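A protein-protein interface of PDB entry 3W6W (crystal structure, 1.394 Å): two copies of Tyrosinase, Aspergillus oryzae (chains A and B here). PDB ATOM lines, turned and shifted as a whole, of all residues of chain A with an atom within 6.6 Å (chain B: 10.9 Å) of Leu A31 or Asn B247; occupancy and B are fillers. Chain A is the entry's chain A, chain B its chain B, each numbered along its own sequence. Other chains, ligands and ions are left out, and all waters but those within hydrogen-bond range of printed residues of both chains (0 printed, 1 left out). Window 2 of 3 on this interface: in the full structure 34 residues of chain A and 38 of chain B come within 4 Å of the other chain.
OD2 of Asp B249 sits at hydrogen-bond distance from OH of Tyr A30.
The guanidinium group (NH1) of Arg A169 lies within hydrogen-bond range of the backbone carbonyl oxygen (O) of Asn B245 (2.9 Å).
Hydrophobic or aromatic side chains of chain B within 4 Å of the printed part of chain A: Tyr B246.
Of the 16 printed residues of chain A, 5 touch a printed residue of chain B.
Hydrophobic or aromatic side chains of chain A within 4 Å of the printed part of chain B: Tyr A30, Leu A31, Ile A172 and Met A176.
Among the printed residues, no Asp or Glu carboxylate lies within 4 Å of a Lys or Arg side-chain nitrogen of the other chain.
CD2 of Leu A31 touches ND2 of Asn B247, 3.5 Å away.
Tyr B246 touches Arg A169.
Asn B247 touches Ile A172.
Asp B249 touches Met A176.
Of chain B, only Asp B249 (2.6 Å) comes within 4 Å of Tyr A30.
Of chain B, only Asn B247 comes within 4 Å of Leu A31.
Arg A157 touches none of the printed residues of chain B.
Of the printed residues of chain B, Arg A169 touches Asn B245 and Tyr B246.
Printed residues of chain B within 4 Å of Ile A172: Asn B247 (3.6 Å).
Printed residues of chain A within 4 Å of Asn B245: Arg A169.
Printed residues of chain A within 4 Å of Asn B247: Leu A31 and Ile A172.
The nearest residue of chain B that does not touch Leu A31 is Asp B249 (7.0 Å).
The nearest printed residue of chain A that does not touch Asn B247 is Tyr A30 (4.1 Å).
The nearest printed residue of chain A that does not touch Tyr B246 is Arg A157 (6.4 Å).
No position is printed for both chains.
Of the 6 pairs that touch across the chains among the printed residues, none has its exchanged pair printed and touching as well.
The backbone NH (N) of Ile A172 is in hydrogen-bond range of the side-chain carboxylate (OD1) of Asp A27, 2.9 Å away.
The backbone carbonyl oxygen (O) of Tyr A30 is in hydrogen-bond range of the side-chain hydroxyl (OG1) of Thr A34 (2.9 Å).
The backbone carbonyl oxygen of Leu A31 lies within hydrogen-bond range of the side-chain hydroxyl of Thr A34 (3.3 Å).
The side-chain amide oxygen (OD1) of Asn B247 lies within hydrogen-bond range of the backbone NH (N) of Asp B249 (2.8 Å).
The side-chain sulfur of Met A176 lies close to the side-chain hydroxyl of Tyr A30, at 3.7 Å.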
ATOM      1  N   ILE A  26      24.116 -12.397 -14.969  1.00  0.00           N
ATOM      2  CA  ILE A  26      24.490 -13.614 -14.256  1.00  0.00           C
ATOM      3  C   ILE A  26      24.780 -13.382 -12.775  1.00  0.00           C
ATOM      4  O   ILE A  26      24.564 -14.273 -11.964  1.00  0.00           O
ATOM      5  CB  ILE A  26      25.679 -14.340 -14.945  1.00  0.00           C
ATOM      6  CG1 ILE A  26      25.814 -15.769 -14.400  1.00  0.00           C
ATOM      7  CG2 ILE A  26      26.973 -13.508 -14.844  1.00  0.00           C
ATOM      8  CD1 ILE A  26      26.791 -16.618 -15.164  1.00  0.00           C
ATOM      9  N   ASP A  27      25.254 -12.191 -12.415  1.00  0.00           N
ATOM     10  CA  ASP A  27      25.416 -11.889 -10.993  1.00  0.00           C
ATOM     11  C   ASP A  27      24.059 -11.701 -10.318  1.00  0.00           C
ATOM     12  O   ASP A  27      23.838 -12.212  -9.220  1.00  0.00           O
ATOM     13  CB  ASP A  27      26.295 -10.648 -10.799  1.00  0.00           C
ATOM     14  CG  ASP A  27      27.780 -10.944 -10.933  1.00  0.00           C
ATOM     15  OD1 ASP A  27      28.155 -12.125 -11.118  1.00  0.00           O
ATOM     16  OD2 ASP A  27      28.566  -9.976 -10.831  1.00  0.00           O
ATOM     17  N   ASP A  28      23.149 -10.975 -10.960  1.00  0.00           N
ATOM     18  CA  ASP A  28      21.829 -10.787 -10.354  1.00  0.00           C
ATOM     19  C   ASP A  28      21.141 -12.131 -10.208  1.00  0.00           C
ATOM     20  O   ASP A  28      20.495 -12.412  -9.197  1.00  0.00           O
ATOM     21  CB  ASP A  28      20.958  -9.867 -11.200  1.00  0.00           C
ATOM     22  CG  ASP A  28      21.412  -8.428 -11.154  1.00  0.00           C
ATOM     23  OD1 ASP A  28      22.148  -8.061 -10.220  1.00  0.00           O
ATOM     24  OD2 ASP A  28      20.996  -7.688 -12.069  1.00  0.00           O
ATOM     25  N   TRP A  29      21.281 -12.959 -11.231  1.00  0.00           N
ATOM     26  CA  TRP A  29      20.663 -14.276 -11.236  1.00  0.00           C
ATOM     27  C   TRP A  29      21.245 -15.176 -10.162  1.00  0.00           C
ATOM     28  O   TRP A  29      20.498 -15.832  -9.428  1.00  0.00           O
ATOM     29  CB  TRP A  29      20.778 -14.897 -12.631  1.00  0.00           C
ATOM     30  CG  TRP A  29      20.339 -16.334 -12.761  1.00  0.00           C
ATOM     31  CD1 TRP A  29      19.062 -16.795 -12.943  1.00  0.00           C
ATOM     32  CD2 TRP A  29      21.184 -17.482 -12.769  1.00  0.00           C
ATOM     33  NE1 TRP A  29      19.068 -18.168 -13.044  1.00  0.00           N
ATOM     34  CE2 TRP A  29      20.359 -18.611 -12.946  1.00  0.00           C
ATOM     35  CE3 TRP A  29      22.563 -17.667 -12.627  1.00  0.00           C
ATOM     36  CZ2 TRP A  29      20.871 -19.906 -12.994  1.00  0.00           C
ATOM     37  CZ3 TRP A  29      23.071 -18.935 -12.682  1.00  0.00           C
ATOM     38  CH2 TRP A  29      22.227 -20.052 -12.863  1.00  0.00           C
ATOM     39  N   TYR A  30      22.567 -15.198 -10.036  1.00  0.00           N
ATOM     40  CA  TYR A  30      23.206 -15.996  -9.003  1.00  0.00           C
ATOM     41  C   TYR A  30      22.767 -15.525  -7.618  1.00  0.00           C
ATOM     42  O   TYR A  30      22.442 -16.342  -6.753  1.00  0.00           O
ATOM     43  CB  TYR A  30      24.743 -15.976  -9.129  1.00  0.00           C
ATOM     44  CG  TYR A  30      25.365 -16.859  -8.082  1.00  0.00           C
ATOM     45  CD1 TYR A  30      25.242 -18.237  -8.166  1.00  0.00           C
ATOM     46  CD2 TYR A  30      26.001 -16.323  -6.962  1.00  0.00           C
ATOM     47  CE1 TYR A  30      25.764 -19.075  -7.198  1.00  0.00           C
ATOM     48  CE2 TYR A  30      26.520 -17.169  -5.967  1.00  0.00           C
ATOM     49  CZ  TYR A  30      26.389 -18.539  -6.096  1.00  0.00           C
ATOM     50  OH  TYR A  30      26.881 -19.406  -5.144  1.00  0.00           O
ATOM     51  N   LEU A  31      22.753 -14.214  -7.406  1.00  0.00           N
ATOM     52  CA  LEU A  31      22.337 -13.657  -6.123  1.00  0.00           C
ATOM     53  C   LEU A  31      20.891 -14.025  -5.842  1.00  0.00           C
ATOM     54  O   LEU A  31      20.567 -14.391  -4.716  1.00  0.00           O
ATOM     55  CB  LEU A  31      22.569 -12.142  -6.094  1.00  0.00           C
ATOM     56  CG  LEU A  31      24.074 -11.818  -6.039  1.00  0.00           C
ATOM     57  CD1 LEU A  31      24.327 -10.339  -6.274  1.00  0.00           C
ATOM     58  CD2 LEU A  31      24.690 -12.252  -4.713  1.00  0.00           C
ATOM     59  N   GLU A  32      20.034 -13.967  -6.860  1.00  0.00           N
ATOM     60  CA  GLU A  32      18.657 -14.364  -6.642  1.00  0.00           C
ATOM     61  C   GLU A  32      18.575 -15.843  -6.273  1.00  0.00           C
ATOM     62  O   GLU A  32      17.934 -16.164  -5.281  1.00  0.00           O
ATOM     63  CB  GLU A  32      17.759 -14.008  -7.826  1.00  0.00           C
ATOM     64  CG  GLU A  32      16.315 -14.431  -7.647  1.00  0.00           C
ATOM     65  CD  GLU A  32      16.076 -15.863  -8.087  1.00  0.00           C
ATOM     66  OE1 GLU A  32      15.295 -16.585  -7.412  1.00  0.00           O
ATOM     67  OE2 GLU A  32      16.689 -16.262  -9.103  1.00  0.00           O
ATOM     68  N   GLN A  33      19.254 -16.713  -7.023  1.00  0.00           N
ATOM     69  CA  GLN A  33      19.240 -18.154  -6.809  1.00  0.00           C
ATOM     70  C   GLN A  33      19.782 -18.590  -5.457  1.00  0.00           C
ATOM     71  O   GLN A  33      19.475 -19.683  -4.998  1.00  0.00           O
ATOM     72  CB  GLN A  33      20.016 -18.861  -7.935  1.00  0.00           C
ATOM     73  CG  GLN A  33      19.317 -18.827  -9.287  1.00  0.00           C
ATOM     74  CD  GLN A  33      18.107 -19.735  -9.306  1.00  0.00           C
ATOM     75  OE1 GLN A  33      18.232 -20.933  -9.058  1.00  0.00           O
ATOM     76  NE2 GLN A  33      16.931 -19.172  -9.595  1.00  0.00           N
ATOM     77  N   THR A  34      20.583 -17.741  -4.823  1.00  0.00           N
ATOM     78  CA  THR A  34      21.185 -18.066  -3.531  1.00  0.00           C
ATOM     79  C   THR A  34      20.584 -17.268  -2.375  1.00  0.00           C
ATOM     80  O   THR A  34      20.967 -17.475  -1.235  1.00  0.00           O
ATOM     81  CB  THR A  34      22.717 -17.862  -3.567  1.00  0.00           C
ATOM     82  OG1 THR A  34      23.021 -16.506  -3.896  1.00  0.00           O
ATOM     83  CG2 THR A  34      23.317 -18.749  -4.631  1.00  0.00           C
ATOM     84  N   SER A  35      19.640 -16.383  -2.696  1.00  0.00           N
ATOM     85  CA  SER A  35      18.962 -15.506  -1.732  1.00  0.00           C
ATOM     86  C   SER A  35      17.904 -16.245  -0.937  1.00  0.00           C
ATOM     87  O   SER A  35      17.384 -17.265  -1.376  1.00  0.00           O
ATOM     88  CB  SER A  35      18.280 -14.340  -2.481  1.00  0.00           C
ATOM     89  OG  SER A  35      17.141 -14.753  -3.257  1.00  0.00           O
ATOM     90  N   ALA A  36      17.573 -15.702   0.230  1.00  0.00           N
ATOM     91  CA  ALA A  36      16.408 -16.179   0.972  1.00  0.00           C
ATOM     92  C   ALA A  36      15.190 -16.036   0.068  1.00  0.00           C
ATOM     93  O   ALA A  36      15.022 -15.012  -0.575  1.00  0.00           O
ATOM     94  CB  ALA A  36      16.218 -15.358   2.232  1.00  0.00           C
ATOM     95  N   SER A  38      14.504 -17.974  -2.627  1.00  0.00           N
ATOM     96  CA  SER A  38      14.675 -18.702  -3.890  1.00  0.00           C
ATOM     97  C   SER A  38      14.678 -20.204  -3.668  1.00  0.00           C
ATOM     98  O   SER A  38      15.032 -20.689  -2.596  1.00  0.00           O
ATOM     99  CB  SER A  38      15.955 -18.292  -4.627  1.00  0.00           C
ATOM    100  OG  SER A  38      16.069 -18.927  -5.902  1.00  0.00           O
ATOM    101  N   ARG A 157      28.135  -5.678  -7.708  1.00  0.00           N
ATOM    102  CA  ARG A 157      27.475  -5.384  -6.433  1.00  0.00           C
ATOM    103  C   ARG A 157      28.370  -5.740  -5.248  1.00  0.00           C
ATOM    104  O   ARG A 157      28.907  -6.847  -5.181  1.00  0.00           O
ATOM    105  CB  ARG A 157      26.144  -6.136  -6.320  1.00  0.00           C
ATOM    106  CG  ARG A 157      25.166  -5.859  -7.448  1.00  0.00           C
ATOM    107  CD  ARG A 157      23.807  -5.396  -6.926  1.00  0.00           C
ATOM    108  NE  ARG A 157      23.246  -6.289  -5.912  1.00  0.00           N
ATOM    109  CZ  ARG A 157      22.465  -7.335  -6.171  1.00  0.00           C
ATOM    110  NH1 ARG A 157      22.146  -7.645  -7.421  1.00  0.00           N
ATOM    111  NH2 ARG A 157      22.003  -8.078  -5.176  1.00  0.00           N
ATOM    112  N   ARG A 169      33.943  -6.496 -12.847  1.00  0.00           N
ATOM    113  CA  ARG A 169      34.407  -7.798 -12.368  1.00  0.00           C
ATOM    114  C   ARG A 169      33.886  -8.914 -13.238  1.00  0.00           C
ATOM    115  O   ARG A 169      32.786  -8.824 -13.786  1.00  0.00           O
ATOM    116  CB  ARG A 169      33.917  -8.105 -10.948  1.00  0.00           C
ATOM    117  CG  ARG A 169      34.444  -7.209  -9.838  1.00  0.00           C
ATOM    118  CD  ARG A 169      33.971  -7.722  -8.494  1.00  0.00           C
ATOM    119  NE  ARG A 169      34.544  -6.936  -7.412  1.00  0.00           N
ATOM    120  CZ  ARG A 169      34.152  -7.021  -6.147  1.00  0.00           C
ATOM    121  NH1 ARG A 169      33.171  -7.846  -5.806  1.00  0.00           N
ATOM    122  NH2 ARG A 169      34.735  -6.278  -5.209  1.00  0.00           N
ATOM    123  N   ILE A 172      30.533 -13.546 -10.434  1.00  0.00           N
ATOM    124  CA  ILE A 172      30.731 -14.291  -9.197  1.00  0.00           C
ATOM    125  C   ILE A 172      30.944 -15.770  -9.498  1.00  0.00           C
ATOM    126  O   ILE A 172      31.913 -16.378  -9.053  1.00  0.00           O
ATOM    127  CB  ILE A 172      29.515 -14.138  -8.260  1.00  0.00           C
ATOM    128  CG1 ILE A 172      29.304 -12.661  -7.903  1.00  0.00           C
ATOM    129  CG2 ILE A 172      29.678 -15.011  -7.006  1.00  0.00           C
ATOM    130  CD1 ILE A 172      27.922 -12.351  -7.344  1.00  0.00           C
ATOM    131  N   MET A 176      34.239 -19.088  -8.727  1.00  0.00           N
ATOM    132  CA  MET A 176      33.966 -20.147  -7.764  1.00  0.00           C
ATOM    133  C   MET A 176      34.367 -21.519  -8.304  1.00  0.00           C
ATOM    134  O   MET A 176      33.716 -22.020  -9.221  1.00  0.00           O
ATOM    135  CB  MET A 176      32.467 -20.155  -7.453  1.00  0.00           C
ATOM    136  CG  MET A 176      31.974 -18.978  -6.620  1.00  0.00           C
ATOM    137  SD  MET A 176      30.171 -18.794  -6.657  1.00  0.00           S
ATOM    138  CE  MET A 176      29.659 -20.485  -6.296  1.00  0.00           C
ATOM    139  N   LEU B 205      31.871 -27.168   3.904  1.00  0.00           N
ATOM    140  CA  LEU B 205      32.588 -26.044   4.511  1.00  0.00           C
ATOM    141  C   LEU B 205      33.102 -26.472   5.883  1.00  0.00           C
ATOM    142  O   LEU B 205      32.399 -27.165   6.611  1.00  0.00           O
ATOM    143  CB  LEU B 205      31.665 -24.832   4.660  1.00  0.00           C
ATOM    144  CG  LEU B 205      31.098 -24.235   3.366  1.00  0.00           C
ATOM    145  CD1 LEU B 205      30.284 -22.990   3.666  1.00  0.00           C
ATOM    146  CD2 LEU B 205      32.203 -23.935   2.362  1.00  0.00           C
ATOM    147  N   PRO B 230      37.443 -15.593   7.455  1.00  0.00           N
ATOM    148  CA  PRO B 230      36.297 -16.506   7.375  1.00  0.00           C
ATOM    149  C   PRO B 230      36.698 -17.935   7.040  1.00  0.00           C
ATOM    150  O   PRO B 230      36.192 -18.525   6.085  1.00  0.00           O
ATOM    151  CB  PRO B 230      35.445 -15.893   6.259  1.00  0.00           C
ATOM    152  CG  PRO B 230      36.428 -15.241   5.363  1.00  0.00           C
ATOM    153  CD  PRO B 230      37.535 -14.714   6.273  1.00  0.00           C
ATOM    154  N   LYS B 233      34.165 -20.561   6.443  1.00  0.00           N
ATOM    155  CA  LYS B 233      33.461 -20.545   5.170  1.00  0.00           C
ATOM    156  C   LYS B 233      34.296 -21.134   4.029  1.00  0.00           C
ATOM    157  O   LYS B 233      33.925 -21.040   2.863  1.00  0.00           O
ATOM    158  CB  LYS B 233      32.992 -19.123   4.868  1.00  0.00           C
ATOM    159  CG  LYS B 233      31.923 -18.675   5.847  1.00  0.00           C
ATOM    160  CD  LYS B 233      31.801 -17.172   5.978  1.00  0.00           C
ATOM    161  CE  LYS B 233      30.517 -16.776   6.702  1.00  0.00           C
ATOM    162  NZ  LYS B 233      30.443 -17.075   8.182  1.00  0.00           N
ATOM    163  N   CYS B 234      35.394 -21.789   4.387  1.00  0.00           N
ATOM    164  CA  CYS B 234      36.257 -22.458   3.415  1.00  0.00           C
ATOM    165  C   CYS B 234      36.029 -23.945   3.432  1.00  0.00           C
ATOM    166  O   CYS B 234      35.931 -24.566   4.506  1.00  0.00           O
ATOM    167  CB  CYS B 234      37.722 -22.258   3.778  1.00  0.00           C
ATOM    168  SG  CYS B 234      38.274 -20.562   3.774  1.00  0.00           S
ATOM    169  N   GLY B 241      43.485 -16.182  -1.060  1.00  0.00           N
ATOM    170  CA  GLY B 241      42.188 -16.240  -1.700  1.00  0.00           C
ATOM    171  C   GLY B 241      41.022 -15.559  -0.993  1.00  0.00           C
ATOM    172  O   GLY B 241      39.958 -15.370  -1.605  1.00  0.00           O
ATOM    173  N   LEU B 242      41.194 -15.195   0.279  1.00  0.00           N
ATOM    174  CA  LEU B 242      40.106 -14.599   1.057  1.00  0.00           C
ATOM    175  C   LEU B 242      40.244 -13.089   1.052  1.00  0.00           C
ATOM    176  O   LEU B 242      41.168 -12.546   1.652  1.00  0.00           O
ATOM    177  CB  LEU B 242      40.126 -15.116   2.503  1.00  0.00           C
ATOM    178  CG  LEU B 242      40.103 -16.642   2.627  1.00  0.00           C
ATOM    179  CD1 LEU B 242      40.097 -17.060   4.098  1.00  0.00           C
ATOM    180  CD2 LEU B 242      38.925 -17.245   1.844  1.00  0.00           C
ATOM    181  N   LEU B 243      39.322 -12.422   0.371  1.00  0.00           N
ATOM    182  CA  LEU B 243      39.297 -10.969   0.310  1.00  0.00           C
ATOM    183  C   LEU B 243      37.905 -10.486   0.659  1.00  0.00           C
ATOM    184  O   LEU B 243      36.904 -11.092   0.266  1.00  0.00           O
ATOM    185  CB  LEU B 243      39.671 -10.447  -1.087  1.00  0.00           C
ATOM    186  CG  LEU B 243      41.133 -10.507  -1.550  1.00  0.00           C
ATOM    187  CD1 LEU B 243      41.440 -11.898  -2.070  1.00  0.00           C
ATOM    188  CD2 LEU B 243      41.376  -9.477  -2.637  1.00  0.00           C
ATOM    189  N   GLU B 244      37.842  -9.384   1.395  1.00  0.00           N
ATOM    190  CA  GLU B 244      36.564  -8.788   1.751  1.00  0.00           C
ATOM    191  C   GLU B 244      35.912  -8.202   0.497  1.00  0.00           C
ATOM    192  O   GLU B 244      36.600  -7.852  -0.461  1.00  0.00           O
ATOM    193  CB  GLU B 244      36.786  -7.701   2.819  1.00  0.00           C
ATOM    194  CG  GLU B 244      35.506  -7.191   3.489  1.00  0.00           C
ATOM    195  CD  GLU B 244      35.779  -6.201   4.616  1.00  0.00           C
ATOM    196  OE1 GLU B 244      36.624  -5.305   4.434  1.00  0.00           O
ATOM    197  OE2 GLU B 244      35.118  -6.303   5.675  1.00  0.00           O
ATOM    198  N   ASN B 245      34.586  -8.125   0.515  1.00  0.00           N
ATOM    199  CA  ASN B 245      33.798  -7.505  -0.551  1.00  0.00           C
ATOM    200  C   ASN B 245      33.743  -8.324  -1.830  1.00  0.00           C
ATOM    201  O   ASN B 245      33.585  -7.788  -2.924  1.00  0.00           O
ATOM    202  CB  ASN B 245      34.233  -6.064  -0.835  1.00  0.00           C
ATOM    203  CG  ASN B 245      33.983  -5.141   0.339  1.00  0.00           C
ATOM    204  OD1 ASN B 245      33.014  -5.303   1.084  1.00  0.00           O
ATOM    205  ND2 ASN B 245      34.857  -4.166   0.511  1.00  0.00           N
ATOM    206  N   TYR B 246      33.862  -9.633  -1.666  1.00  0.00           N
ATOM    207  CA  TYR B 246      33.510 -10.590  -2.711  1.00  0.00           C
ATOM    208  C   TYR B 246      32.466 -11.499  -2.104  1.00  0.00           C
ATOM    209  O   TYR B 246      32.358 -11.605  -0.882  1.00  0.00           O
ATOM    210  CB  TYR B 246      34.731 -11.387  -3.172  1.00  0.00           C
ATOM    211  CG  TYR B 246      35.729 -10.479  -3.817  1.00  0.00           C
ATOM    212  CD1 TYR B 246      35.646 -10.164  -5.169  1.00  0.00           C
ATOM    213  CD2 TYR B 246      36.710  -9.863  -3.055  1.00  0.00           C
ATOM    214  CE1 TYR B 246      36.552  -9.291  -5.747  1.00  0.00           C
ATOM    215  CE2 TYR B 246      37.612  -8.986  -3.616  1.00  0.00           C
ATOM    216  CZ  TYR B 246      37.536  -8.707  -4.966  1.00  0.00           C
ATOM    217  OH  TYR B 246      38.457  -7.826  -5.489  1.00  0.00           O
ATOM    218  N   ASN B 247      31.681 -12.142  -2.954  1.00  0.00           N
ATOM    219  CA  ASN B 247      30.634 -13.036  -2.482  1.00  0.00           C
ATOM    220  C   ASN B 247      31.218 -14.151  -1.610  1.00  0.00           C
ATOM    221  O   ASN B 247      32.265 -14.722  -1.921  1.00  0.00           O
ATOM    222  CB  ASN B 247      29.915 -13.623  -3.691  1.00  0.00           C
ATOM    223  CG  ASN B 247      28.700 -14.426  -3.308  1.00  0.00           C
ATOM    224  OD1 ASN B 247      28.822 -15.582  -2.912  1.00  0.00           O
ATOM    225  ND2 ASN B 247      27.531 -13.844  -3.461  1.00  0.00           N
ATOM    226  N   ALA B 248      30.546 -14.458  -0.504  1.00  0.00           N
ATOM    227  CA  ALA B 248      31.095 -15.429   0.433  1.00  0.00           C
ATOM    228  C   ALA B 248      31.259 -16.822  -0.161  1.00  0.00           C
ATOM    229  O   ALA B 248      32.088 -17.605   0.307  1.00  0.00           O
ATOM    230  CB  ALA B 248      30.246 -15.496   1.701  1.00  0.00           C
ATOM    231  N   ASP B 249      30.499 -17.124  -1.214  1.00  0.00           N
ATOM    232  CA  ASP B 249      30.656 -18.417  -1.875  1.00  0.00           C
ATOM    233  C   ASP B 249      31.986 -18.550  -2.609  1.00  0.00           C
ATOM    234  O   ASP B 249      32.430 -19.645  -2.860  1.00  0.00           O
ATOM    235  CB  ASP B 249      29.471 -18.722  -2.794  1.00  0.00           C
ATOM    236  CG  ASP B 249      28.164 -18.777  -2.043  1.00  0.00           C
ATOM    237  OD1 ASP B 249      28.182 -19.031  -0.812  1.00  0.00           O
ATOM    238  OD2 ASP B 249      27.122 -18.537  -2.663  1.00  0.00           O
ATOM    239  N   VAL B 250      32.641 -17.425  -2.874  1.00  0.00           N
ATOM    240  CA  VAL B 250      33.971 -17.448  -3.463  1.00  0.00           C
ATOM    241  C   VAL B 250      34.966 -18.026  -2.466  1.00  0.00           C
ATOM    242  O   VAL B 250      35.942 -18.661  -2.845  1.00  0.00           O
ATOM    243  CB  VAL B 250      34.398 -16.028  -3.921  1.00  0.00           C
ATOM    244  CG1 VAL B 250      35.844 -16.018  -4.453  1.00  0.00           C
ATOM    245  CG2 VAL B 250      33.443 -15.514  -4.979  1.00  0.00           C
ATOM    246  N   TRP B 251      34.702 -17.822  -1.180  1.00  0.00           N
ATOM    247  CA  TRP B 251      35.624 -18.262  -0.132  1.00  0.00           C
ATOM    248  C   TRP B 251      35.654 -19.777   0.058  1.00  0.00           C
ATOM    249  O   TRP B 251      36.583 -20.305   0.676  1.00  0.00           O
ATOM    250  CB  TRP B 251      35.284 -17.580   1.196  1.00  0.00           C
ATOM    251  CG  TRP B 251      35.327 -16.083   1.144  1.00  0.00           C
ATOM    252  CD1 TRP B 251      36.065 -15.295   0.286  1.00  0.00           C
ATOM    253  CD2 TRP B 251      34.577 -15.189   1.965  1.00  0.00           C
ATOM    254  NE1 TRP B 251      35.812 -13.967   0.538  1.00  0.00           N
ATOM    255  CE2 TRP B 251      34.911 -13.874   1.572  1.00  0.00           C
ATOM    256  CE3 TRP B 251      33.666 -15.372   3.016  1.00  0.00           C
ATOM    257  CZ2 TRP B 251      34.338 -12.752   2.170  1.00  0.00           C
ATOM    258  CZ3 TRP B 251      33.101 -14.266   3.608  1.00  0.00           C
ATOM    259  CH2 TRP B 251      33.446 -12.965   3.193  1.00  0.00           C
ATOM    260  N   ALA B 252      34.660 -20.478  -0.479  1.00  0.00           N
ATOM    261  CA  ALA B 252      34.611 -21.929  -0.325  1.00  0.00           C
ATOM    262  C   ALA B 252      35.905 -22.536  -0.836  1.00  0.00           C
ATOM    263  O   ALA B 252      36.487 -23.413  -0.197  1.00  0.00           O
ATOM    264  CB  ALA B 252      33.413 -22.514  -1.047  1.00  0.00           C
ATOM    265  N   ASP B 253      36.370 -22.033  -1.978  1.00  0.00           N
ATOM    266  CA  ASP B 253      37.704 -22.359  -2.501  1.00  0.00           C
ATOM    267  C   ASP B 253      38.287 -21.083  -3.110  1.00  0.00           C
ATOM    268  O   ASP B 253      37.974 -20.726  -4.249  1.00  0.00           O
ATOM    269  CB  ASP B 253      37.620 -23.480  -3.548  1.00  0.00           C
ATOM    270  CG  ASP B 253      38.989 -23.890  -4.103  1.00  0.00           C
ATOM    271  OD1 ASP B 253      40.014 -23.266  -3.742  1.00  0.00           O
ATOM    272  OD2 ASP B 253      39.022 -24.824  -4.938  1.00  0.00           O
ATOM    273  N   GLY B 254      39.121 -20.386  -2.345  1.00  0.00           N
ATOM    274  CA  GLY B 254      39.722 -19.144  -2.796  1.00  0.00           C
ATOM    275  C   GLY B 254      40.869 -19.309  -3.781  1.00  0.00           C
ATOM    276  O   GLY B 254      41.397 -18.322  -4.282  1.00  0.00           O
ATOM    277  N   PHE B 344      42.897  -9.520   4.883  1.00  0.00           N
ATOM    278  CA  PHE B 344      41.590  -9.756   4.280  1.00  0.00           C
ATOM    279  C   PHE B 344      41.104  -8.535   3.512  1.00  0.00           C
ATOM    280  O   PHE B 344      40.307  -8.649   2.588  1.00  0.00           O
ATOM    281  CB  PHE B 344      40.634 -10.068   5.433  1.00  0.00           C
ATOM    282  CG  PHE B 344      39.241 -10.480   5.030  1.00  0.00           C
ATOM    283  CD1 PHE B 344      39.010 -11.546   4.166  1.00  0.00           C
ATOM    284  CD2 PHE B 344      38.156  -9.835   5.592  1.00  0.00           C
ATOM    285  CE1 PHE B 344      37.717 -11.924   3.860  1.00  0.00           C
ATOM    286  CE2 PHE B 344      36.866 -10.215   5.284  1.00  0.00           C
ATOM    287  CZ  PHE B 344      36.646 -11.259   4.414  1.00  0.00           C
